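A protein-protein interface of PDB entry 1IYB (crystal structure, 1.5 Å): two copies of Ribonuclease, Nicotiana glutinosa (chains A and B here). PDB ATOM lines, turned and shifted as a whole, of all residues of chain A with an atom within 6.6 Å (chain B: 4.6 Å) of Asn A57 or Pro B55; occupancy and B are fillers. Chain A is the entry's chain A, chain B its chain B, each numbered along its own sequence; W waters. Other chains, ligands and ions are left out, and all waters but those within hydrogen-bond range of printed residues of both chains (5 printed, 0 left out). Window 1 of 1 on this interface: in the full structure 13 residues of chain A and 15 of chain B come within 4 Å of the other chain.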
ATOM      1  N   PRO A  55     -21.389 -17.631 -23.685  1.00  0.00           N
ATOM      2  CA  PRO A  55     -19.950 -17.787 -23.468  1.00  0.00           C
ATOM      3  C   PRO A  55     -19.409 -18.778 -24.498  1.00  0.00           C
ATOM      4  O   PRO A  55     -20.153 -19.620 -24.996  1.00  0.00           O
ATOM      5  CB  PRO A  55     -19.880 -18.344 -22.056  1.00  0.00           C
ATOM      6  CG  PRO A  55     -21.107 -19.217 -21.997  1.00  0.00           C
ATOM      7  CD  PRO A  55     -22.163 -18.358 -22.662  1.00  0.00           C
ATOM      8  N   SER A  56     -18.128 -18.664 -24.832  1.00  0.00           N
ATOM      9  CA  SER A  56     -17.512 -19.593 -25.780  1.00  0.00           C
ATOM     10  C   SER A  56     -16.021 -19.755 -25.505  1.00  0.00           C
ATOM     11  O   SER A  56     -15.361 -18.808 -25.083  1.00  0.00           O
ATOM     12  CB  SER A  56     -17.734 -19.135 -27.230  1.00  0.00           C
ATOM     13  OG  SER A  56     -17.220 -17.837 -27.462  1.00  0.00           O
ATOM     14  N   ASN A  57     -15.513 -20.969 -25.739  1.00  0.00           N
ATOM     15  CA  ASN A  57     -14.103 -21.322 -25.536  1.00  0.00           C
ATOM     16  C   ASN A  57     -13.677 -20.926 -24.131  1.00  0.00           C
ATOM     17  O   ASN A  57     -12.751 -20.143 -23.944  1.00  0.00           O
ATOM     18  CB  ASN A  57     -13.220 -20.608 -26.560  1.00  0.00           C
ATOM     19  CG  ASN A  57     -13.639 -20.891 -27.988  1.00  0.00           C
ATOM     20  OD1 ASN A  57     -14.036 -19.985 -28.721  1.00  0.00           O
ATOM     21  ND2 ASN A  57     -13.550 -22.152 -28.394  1.00  0.00           N
ATOM     22  N   CYS A  58     -14.346 -21.515 -23.147  1.00  0.00           N
ATOM     23  CA  CYS A  58     -14.128 -21.195 -21.744  1.00  0.00           C
ATOM     24  C   CYS A  58     -12.955 -21.798 -20.969  1.00  0.00           C
ATOM     25  O   CYS A  58     -12.642 -21.309 -19.882  1.00  0.00           O
ATOM     26  CB  CYS A  58     -15.425 -21.476 -20.981  1.00  0.00           C
ATOM     27  SG  CYS A  58     -16.831 -20.455 -21.549  1.00  0.00           S
ATOM     28  N   ASP A  59     -12.305 -22.836 -21.487  1.00  0.00           N
ATOM     29  CA  ASP A  59     -11.189 -23.430 -20.746  1.00  0.00           C
ATOM     30  C   ASP A  59     -10.142 -24.078 -21.644  1.00  0.00           C
ATOM     31  O   ASP A  59     -10.278 -25.234 -22.050  1.00  0.00           O
ATOM     32  CB  ASP A  59     -11.711 -24.469 -19.752  1.00  0.00           C
ATOM     33  CG  ASP A  59     -10.676 -24.845 -18.699  1.00  0.00           C
ATOM     34  OD1 ASP A  59      -9.468 -24.597 -18.919  1.00  0.00           O
ATOM     35  OD2 ASP A  59     -11.071 -25.396 -17.649  1.00  0.00           O
ATOM     36  N   SER A  60      -9.082 -23.332 -21.928  1.00  0.00           N
ATOM     37  CA  SER A  60      -8.009 -23.816 -22.788  1.00  0.00           C
ATOM     38  C   SER A  60      -7.247 -25.001 -22.202  1.00  0.00           C
ATOM     39  O   SER A  60      -6.519 -25.688 -22.919  1.00  0.00           O
ATOM     40  CB  SER A  60      -7.023 -22.681 -23.068  1.00  0.00           C
ATOM     41  OG  SER A  60      -6.407 -22.252 -21.866  1.00  0.00           O
ATOM     42  N   HIS A  96     -14.526 -29.756 -31.496  1.00  0.00           N
ATOM     43  CA  HIS A  96     -14.921 -28.358 -31.615  1.00  0.00           C
ATOM     44  C   HIS A  96     -16.086 -28.023 -30.684  1.00  0.00           C
ATOM     45  O   HIS A  96     -16.081 -26.992 -30.012  1.00  0.00           O
ATOM     46  CB  HIS A  96     -15.317 -28.048 -33.063  1.00  0.00           C
ATOM     47  CG  HIS A  96     -15.944 -26.702 -33.240  1.00  0.00           C
ATOM     48  ND1 HIS A  96     -15.223 -25.530 -33.178  1.00  0.00           N
ATOM     49  CD2 HIS A  96     -17.234 -26.340 -33.441  1.00  0.00           C
ATOM     50  CE1 HIS A  96     -16.040 -24.503 -33.335  1.00  0.00           C
ATOM     51  NE2 HIS A  96     -17.267 -24.967 -33.495  1.00  0.00           N
ATOM     52  N   GLU A  99     -14.753 -28.034 -26.965  1.00  0.00           N
ATOM     53  CA  GLU A  99     -13.900 -26.893 -26.668  1.00  0.00           C
ATOM     54  C   GLU A  99     -14.596 -25.540 -26.725  1.00  0.00           C
ATOM     55  O   GLU A  99     -14.343 -24.675 -25.887  1.00  0.00           O
ATOM     56  CB  GLU A  99     -12.670 -26.934 -27.578  1.00  0.00           C
ATOM     57  CG  GLU A  99     -11.871 -28.212 -27.340  1.00  0.00           C
ATOM     58  CD  GLU A  99     -10.487 -28.204 -27.956  1.00  0.00           C
ATOM     59  OE1 GLU A  99      -9.762 -29.209 -27.764  1.00  0.00           O
ATOM     60  OE2 GLU A  99     -10.124 -27.209 -28.624  1.00  0.00           O
ATOM     61  N   LYS A 100     -15.493 -25.350 -27.685  1.00  0.00           N
ATOM     62  CA  LYS A 100     -16.197 -24.074 -27.789  1.00  0.00           C
ATOM     63  C   LYS A 100     -17.378 -23.941 -26.831  1.00  0.00           C
ATOM     64  O   LYS A 100     -17.598 -22.875 -26.250  1.00  0.00           O
ATOM     65  CB  LYS A 100     -16.707 -23.849 -29.216  1.00  0.00           C
ATOM     66  CG  LYS A 100     -17.497 -22.548 -29.381  1.00  0.00           C
ATOM     67  CD  LYS A 100     -17.904 -22.298 -30.830  1.00  0.00           C
ATOM     68  CE  LYS A 100     -18.619 -20.954 -30.979  1.00  0.00           C
ATOM     69  NZ  LYS A 100     -19.003 -20.648 -32.391  1.00  0.00           N
ATOM     70  N   HIS A 101     -18.132 -25.023 -26.658  1.00  0.00           N
ATOM     71  CA  HIS A 101     -19.324 -24.991 -25.813  1.00  0.00           C
ATOM     72  C   HIS A 101     -19.269 -25.801 -24.512  1.00  0.00           C
ATOM     73  O   HIS A 101     -19.622 -25.300 -23.442  1.00  0.00           O
ATOM     74  CB  HIS A 101     -20.525 -25.449 -26.644  1.00  0.00           C
ATOM     75  CG  HIS A 101     -20.835 -24.558 -27.811  1.00  0.00           C
ATOM     76  ND1 HIS A 101     -21.345 -23.286 -27.660  1.00  0.00           N
ATOM     77  CD2 HIS A 101     -20.725 -24.762 -29.146  1.00  0.00           C
ATOM     78  CE1 HIS A 101     -21.538 -22.747 -28.852  1.00  0.00           C
ATOM     79  NE2 HIS A 101     -21.171 -23.622 -29.770  1.00  0.00           N
ATOM     80  N   THR A 103     -16.834 -26.741 -22.581  1.00  0.00           N
ATOM     81  CA  THR A 103     -15.992 -26.166 -21.541  1.00  0.00           C
ATOM     82  C   THR A 103     -16.709 -25.073 -20.749  1.00  0.00           C
ATOM     83  O   THR A 103     -16.351 -24.790 -19.603  1.00  0.00           O
ATOM     84  CB  THR A 103     -14.705 -25.570 -22.139  1.00  0.00           C
ATOM     85  OG1 THR A 103     -15.051 -24.575 -23.113  1.00  0.00           O
ATOM     86  CG2 THR A 103     -13.861 -26.665 -22.793  1.00  0.00           C
ATOM     87  N   CYS A 104     -17.719 -24.458 -21.357  1.00  0.00           N
ATOM     88  CA  CYS A 104     -18.456 -23.396 -20.685  1.00  0.00           C
ATOM     89  C   CYS A 104     -19.496 -23.927 -19.702  1.00  0.00           C
ATOM     90  O   CYS A 104     -20.195 -23.148 -19.050  1.00  0.00           O
ATOM     91  CB  CYS A 104     -19.110 -22.476 -21.722  1.00  0.00           C
ATOM     92  SG  CYS A 104     -17.900 -21.650 -22.815  1.00  0.00           S
ATOM     93  N   PHE B   8      -7.440 -19.410 -19.892  1.00  0.00           N
ATOM     94  CA  PHE B   8      -6.982 -18.952 -21.196  1.00  0.00           C
ATOM     95  C   PHE B   8      -5.459 -18.909 -21.121  1.00  0.00           C
ATOM     96  O   PHE B   8      -4.890 -18.996 -20.032  1.00  0.00           O
ATOM     97  CB  PHE B   8      -7.588 -17.582 -21.544  1.00  0.00           C
ATOM     98  CG  PHE B   8      -7.150 -16.472 -20.642  1.00  0.00           C
ATOM     99  CD1 PHE B   8      -6.058 -15.681 -20.975  1.00  0.00           C
ATOM    100  CD2 PHE B   8      -7.811 -16.234 -19.443  1.00  0.00           C
ATOM    101  CE1 PHE B   8      -5.629 -14.669 -20.123  1.00  0.00           C
ATOM    102  CE2 PHE B   8      -7.390 -15.226 -18.588  1.00  0.00           C
ATOM    103  CZ  PHE B   8      -6.296 -14.443 -18.929  1.00  0.00           C
ATOM    104  N   PRO B  47      -8.049 -11.700 -23.956  1.00  0.00           N
ATOM    105  CA  PRO B  47      -7.515 -13.014 -23.588  1.00  0.00           C
ATOM    106  C   PRO B  47      -7.535 -13.840 -24.884  1.00  0.00           C
ATOM    107  O   PRO B  47      -8.469 -13.713 -25.689  1.00  0.00           O
ATOM    108  CB  PRO B  47      -8.537 -13.523 -22.573  1.00  0.00           C
ATOM    109  CG  PRO B  47      -8.960 -12.272 -21.876  1.00  0.00           C
ATOM    110  CD  PRO B  47      -9.131 -11.293 -23.038  1.00  0.00           C
ATOM    111  N   ASN B  48      -6.511 -14.662 -25.100  1.00  0.00           N
ATOM    112  CA  ASN B  48      -6.424 -15.479 -26.314  1.00  0.00           C
ATOM    113  C   ASN B  48      -5.721 -16.784 -25.977  1.00  0.00           C
ATOM    114  O   ASN B  48      -5.029 -16.880 -24.961  1.00  0.00           O
ATOM    115  CB  ASN B  48      -5.625 -14.746 -27.398  1.00  0.00           C
ATOM    116  CG  ASN B  48      -6.015 -15.171 -28.811  1.00  0.00           C
ATOM    117  OD1 ASN B  48      -6.987 -14.668 -29.374  1.00  0.00           O
ATOM    118  ND2 ASN B  48      -5.258 -16.101 -29.388  1.00  0.00           N
ATOM    119  N   ASN B  49      -5.884 -17.782 -26.840  1.00  0.00           N
ATOM    120  CA  ASN B  49      -5.289 -19.089 -26.605  1.00  0.00           C
ATOM    121  C   ASN B  49      -4.204 -19.472 -27.608  1.00  0.00           C
ATOM    122  O   ASN B  49      -4.138 -18.931 -28.715  1.00  0.00           O
ATOM    123  CB  ASN B  49      -6.403 -20.135 -26.585  1.00  0.00           C
ATOM    124  CG  ASN B  49      -7.381 -19.902 -25.449  1.00  0.00           C
ATOM    125  OD1 ASN B  49      -8.585 -20.128 -25.584  1.00  0.00           O
ATOM    126  ND2 ASN B  49      -6.863 -19.450 -24.316  1.00  0.00           N
ATOM    127  N   SER B  53      -7.833 -19.891 -30.710  1.00  0.00           N
ATOM    128  CA  SER B  53      -9.175 -19.614 -30.220  1.00  0.00           C
ATOM    129  C   SER B  53      -9.074 -18.557 -29.131  1.00  0.00           C
ATOM    130  O   SER B  53      -7.978 -18.193 -28.699  1.00  0.00           O
ATOM    131  CB  SER B  53      -9.803 -20.876 -29.625  1.00  0.00           C
ATOM    132  OG  SER B  53      -9.139 -21.254 -28.428  1.00  0.00           O
ATOM    133  N   TYR B  54     -10.219 -18.056 -28.691  1.00  0.00           N
ATOM    134  CA  TYR B  54     -10.233 -17.069 -27.620  1.00  0.00           C
ATOM    135  C   TYR B  54     -11.560 -17.127 -26.907  1.00  0.00           C
ATOM    136  O   TYR B  54     -12.589 -17.391 -27.523  1.00  0.00           O
ATOM    137  CB  TYR B  54      -9.979 -15.653 -28.158  1.00  0.00           C
ATOM    138  CG  TYR B  54     -10.999 -15.140 -29.147  1.00  0.00           C
ATOM    139  CD1 TYR B  54     -12.205 -14.582 -28.718  1.00  0.00           C
ATOM    140  CD2 TYR B  54     -10.750 -15.204 -30.518  1.00  0.00           C
ATOM    141  CE1 TYR B  54     -13.141 -14.095 -29.637  1.00  0.00           C
ATOM    142  CE2 TYR B  54     -11.673 -14.724 -31.442  1.00  0.00           C
ATOM    143  CZ  TYR B  54     -12.864 -14.170 -30.997  1.00  0.00           C
ATOM    144  OH  TYR B  54     -13.771 -13.687 -31.915  1.00  0.00           O
ATOM    145  N   PRO B  55     -11.549 -16.919 -25.585  1.00  0.00           N
ATOM    146  CA  PRO B  55     -12.790 -16.949 -24.809  1.00  0.00           C
ATOM    147  C   PRO B  55     -13.535 -15.636 -25.043  1.00  0.00           C
ATOM    148  O   PRO B  55     -12.915 -14.609 -25.324  1.00  0.00           O
ATOM    149  CB  PRO B  55     -12.286 -17.067 -23.378  1.00  0.00           C
ATOM    150  CG  PRO B  55     -11.037 -16.220 -23.415  1.00  0.00           C
ATOM    151  CD  PRO B  55     -10.386 -16.658 -24.715  1.00  0.00           C
ATOM    152  N   SER B  56     -14.858 -15.669 -24.954  1.00  0.00           N
ATOM    153  CA  SER B  56     -15.640 -14.449 -25.125  1.00  0.00           C
ATOM    154  C   SER B  56     -16.942 -14.519 -24.330  1.00  0.00           C
ATOM    155  O   SER B  56     -17.504 -15.599 -24.133  1.00  0.00           O
ATOM    156  CB  SER B  56     -15.938 -14.187 -26.607  1.00  0.00           C
ATOM    157  OG  SER B  56     -16.718 -15.218 -27.177  1.00  0.00           O
ATOM    158  N   CYS B  58     -17.706 -14.193 -21.089  1.00  0.00           N
ATOM    159  CA  CYS B  58     -17.595 -15.129 -19.984  1.00  0.00           C
ATOM    160  C   CYS B  58     -18.429 -14.852 -18.733  1.00  0.00           C
ATOM    161  O   CYS B  58     -18.486 -15.698 -17.839  1.00  0.00           O
ATOM    162  CB  CYS B  58     -16.114 -15.264 -19.609  1.00  0.00           C
ATOM    163  SG  CYS B  58     -15.076 -15.875 -20.982  1.00  0.00           S
ATOM    164  N   LYS B 100     -17.326  -8.483 -23.537  1.00  0.00           N
ATOM    165  CA  LYS B 100     -16.817  -9.516 -24.432  1.00  0.00           C
ATOM    166  C   LYS B 100     -15.462 -10.111 -24.055  1.00  0.00           C
ATOM    167  O   LYS B 100     -15.280 -11.328 -24.098  1.00  0.00           O
ATOM    168  CB  LYS B 100     -16.748  -8.980 -25.868  1.00  0.00           C
ATOM    169  CG  LYS B 100     -16.188  -9.978 -26.876  1.00  0.00           C
ATOM    170  CD  LYS B 100     -16.236  -9.439 -28.296  1.00  0.00           C
ATOM    171  CE  LYS B 100     -15.715 -10.480 -29.275  1.00  0.00           C
ATOM    172  NZ  LYS B 100     -15.903 -10.053 -30.691  1.00  0.00           N
ATOM    173  N   CYS B 104     -13.690 -12.397 -19.348  1.00  0.00           N
ATOM    174  CA  CYS B 104     -12.968 -13.652 -19.485  1.00  0.00           C
ATOM    175  C   CYS B 104     -11.659 -13.681 -18.709  1.00  0.00           C
ATOM    176  O   CYS B 104     -11.009 -14.720 -18.609  1.00  0.00           O
ATOM    177  CB  CYS B 104     -12.727 -13.949 -20.964  1.00  0.00           C
ATOM    178  SG  CYS B 104     -14.291 -14.204 -21.867  1.00  0.00           S
HETATM  179  O   HOH W   1     -19.301 -15.825 -27.462  1.00  0.00           O
HETATM  180  O   HOH W   2     -10.114 -20.025 -23.177  1.00  0.00           O
HETATM  181  O   HOH W   3     -14.999 -16.883 -28.612  1.00  0.00           O
HETATM  182  O   HOH W   4     -12.315 -18.316 -31.005  1.00  0.00           O
HETATM  183  O   HOH W   5     -13.730 -18.844 -19.080  1.00  0.00           O
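The side-chain hydroxyl (OG) of Ser A56 sits at hydrogen-bond distance from the side-chain hydroxyl (OG) of Ser B56 (2.7 Å).
O of Tyr B54 lies close to OD1 of Asn A57, at 3.2 Å.
The backbone NH (N) of Ser A56 is in hydrogen-bond range of the side-chain sulfur (SG) of Cys A104, 3.6 Å away.
N of Asn A57 lies within hydrogen-bond range of O of Lys A100 (2.9 Å).
The side-chain hydroxyl (OG) of Ser B53 sits at hydrogen-bond distance from the side-chain amide oxygen (OD1) of Asn B49 (3.1 Å).
N of Ser B56 lies within hydrogen-bond range of SG of Cys B104 (3.5 Å).
SG of Cys A58 forms a disulfide with SG of Cys A104 (2.0 Å).
SG of Cys B58 forms a disulfide with SG of Cys B104 (2.0 Å).
O of Ser B56 touches CA of Pro A55, at 3.3 Å.
Tyr B54 touches Ser A56.
CA of Pro B55 touches O of Ser A56 (3.2 Å).
O of Asn A57 touches CB of Pro B55 (3.2 Å).
OG of Ser A60 touches CA of Phe B8, 3.4 Å away.
Asn B49 touches Ser A60.
Asn A57 touches two residues of chain B.
Pro B55 touches two residues of chain A.
Of the printed residues of chain B, Pro A55 touches Ser B56 (3.3 Å).
Of the printed residues of chain B, Ser A60 touches Phe B8 (3.4 Å) and Asn B49 (3.5 Å).
Printed residues of chain B within 4 Å of Ser A56: Tyr B54 (3.96 Å), Pro B55 (3.2 Å) and Ser B56 (2.7 Å).
Of the printed residues of chain A, Asn B49 touches Ser A60.
The nearest residue of chain A that does not touch Pro B55 is Cys A58 (4.8 Å).
The nearest printed residue of chain A that does not touch Asn B49 is Asn A57 (4.5 Å).
Printed residues of chain A that touch a printed residue of chain B: Pro A55, Ser A56, Asn A57 and Ser A60.
Along chain A the printed residues that touch a printed residue of chain B span positions 55 to 60.
Of the 11 printed residues of chain B, 5 touch a printed residue of chain A.
Hydrophobic or aromatic side chains of chain B within 4 Å of the printed part of chain A: Pro B55.
Pro A55 touches Ser B56, and with the chains exchanged Ser A56 touches Pro B55.
Ser A56 touches its own counterpart, Ser B56.
Water W1 lies within hydrogen-bond range of the side-chain hydroxyl (OG) of Ser B56 (2.7 Å) and the side-chain hydroxyl (OG) of Ser A56 (2.9 Å).
Water W3 lies within hydrogen-bond range of the side-chain hydroxyl (OG) of Ser A56 (2.7 Å), the backbone carbonyl oxygen (O) of Tyr B54 (2.7 Å), the side-chain hydroxyl (OG) of Ser B56 (2.8 Å) and the side-chain amide oxygen (OD1) of Asn A57 (3.2 Å).
Water W2 bridges O of Asn A57 (2.7 Å) and OD1 of Asn B49 (2.9 Å).
Water W5 lies within hydrogen-bond range of O of Cys A58 (2.8 Å) and SG of Cys B58 (3.8 Å).
Water W4 bridges the backbone NH (N) of Tyr B54 and the side-chain amide oxygen (OD1) of Asn A57.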
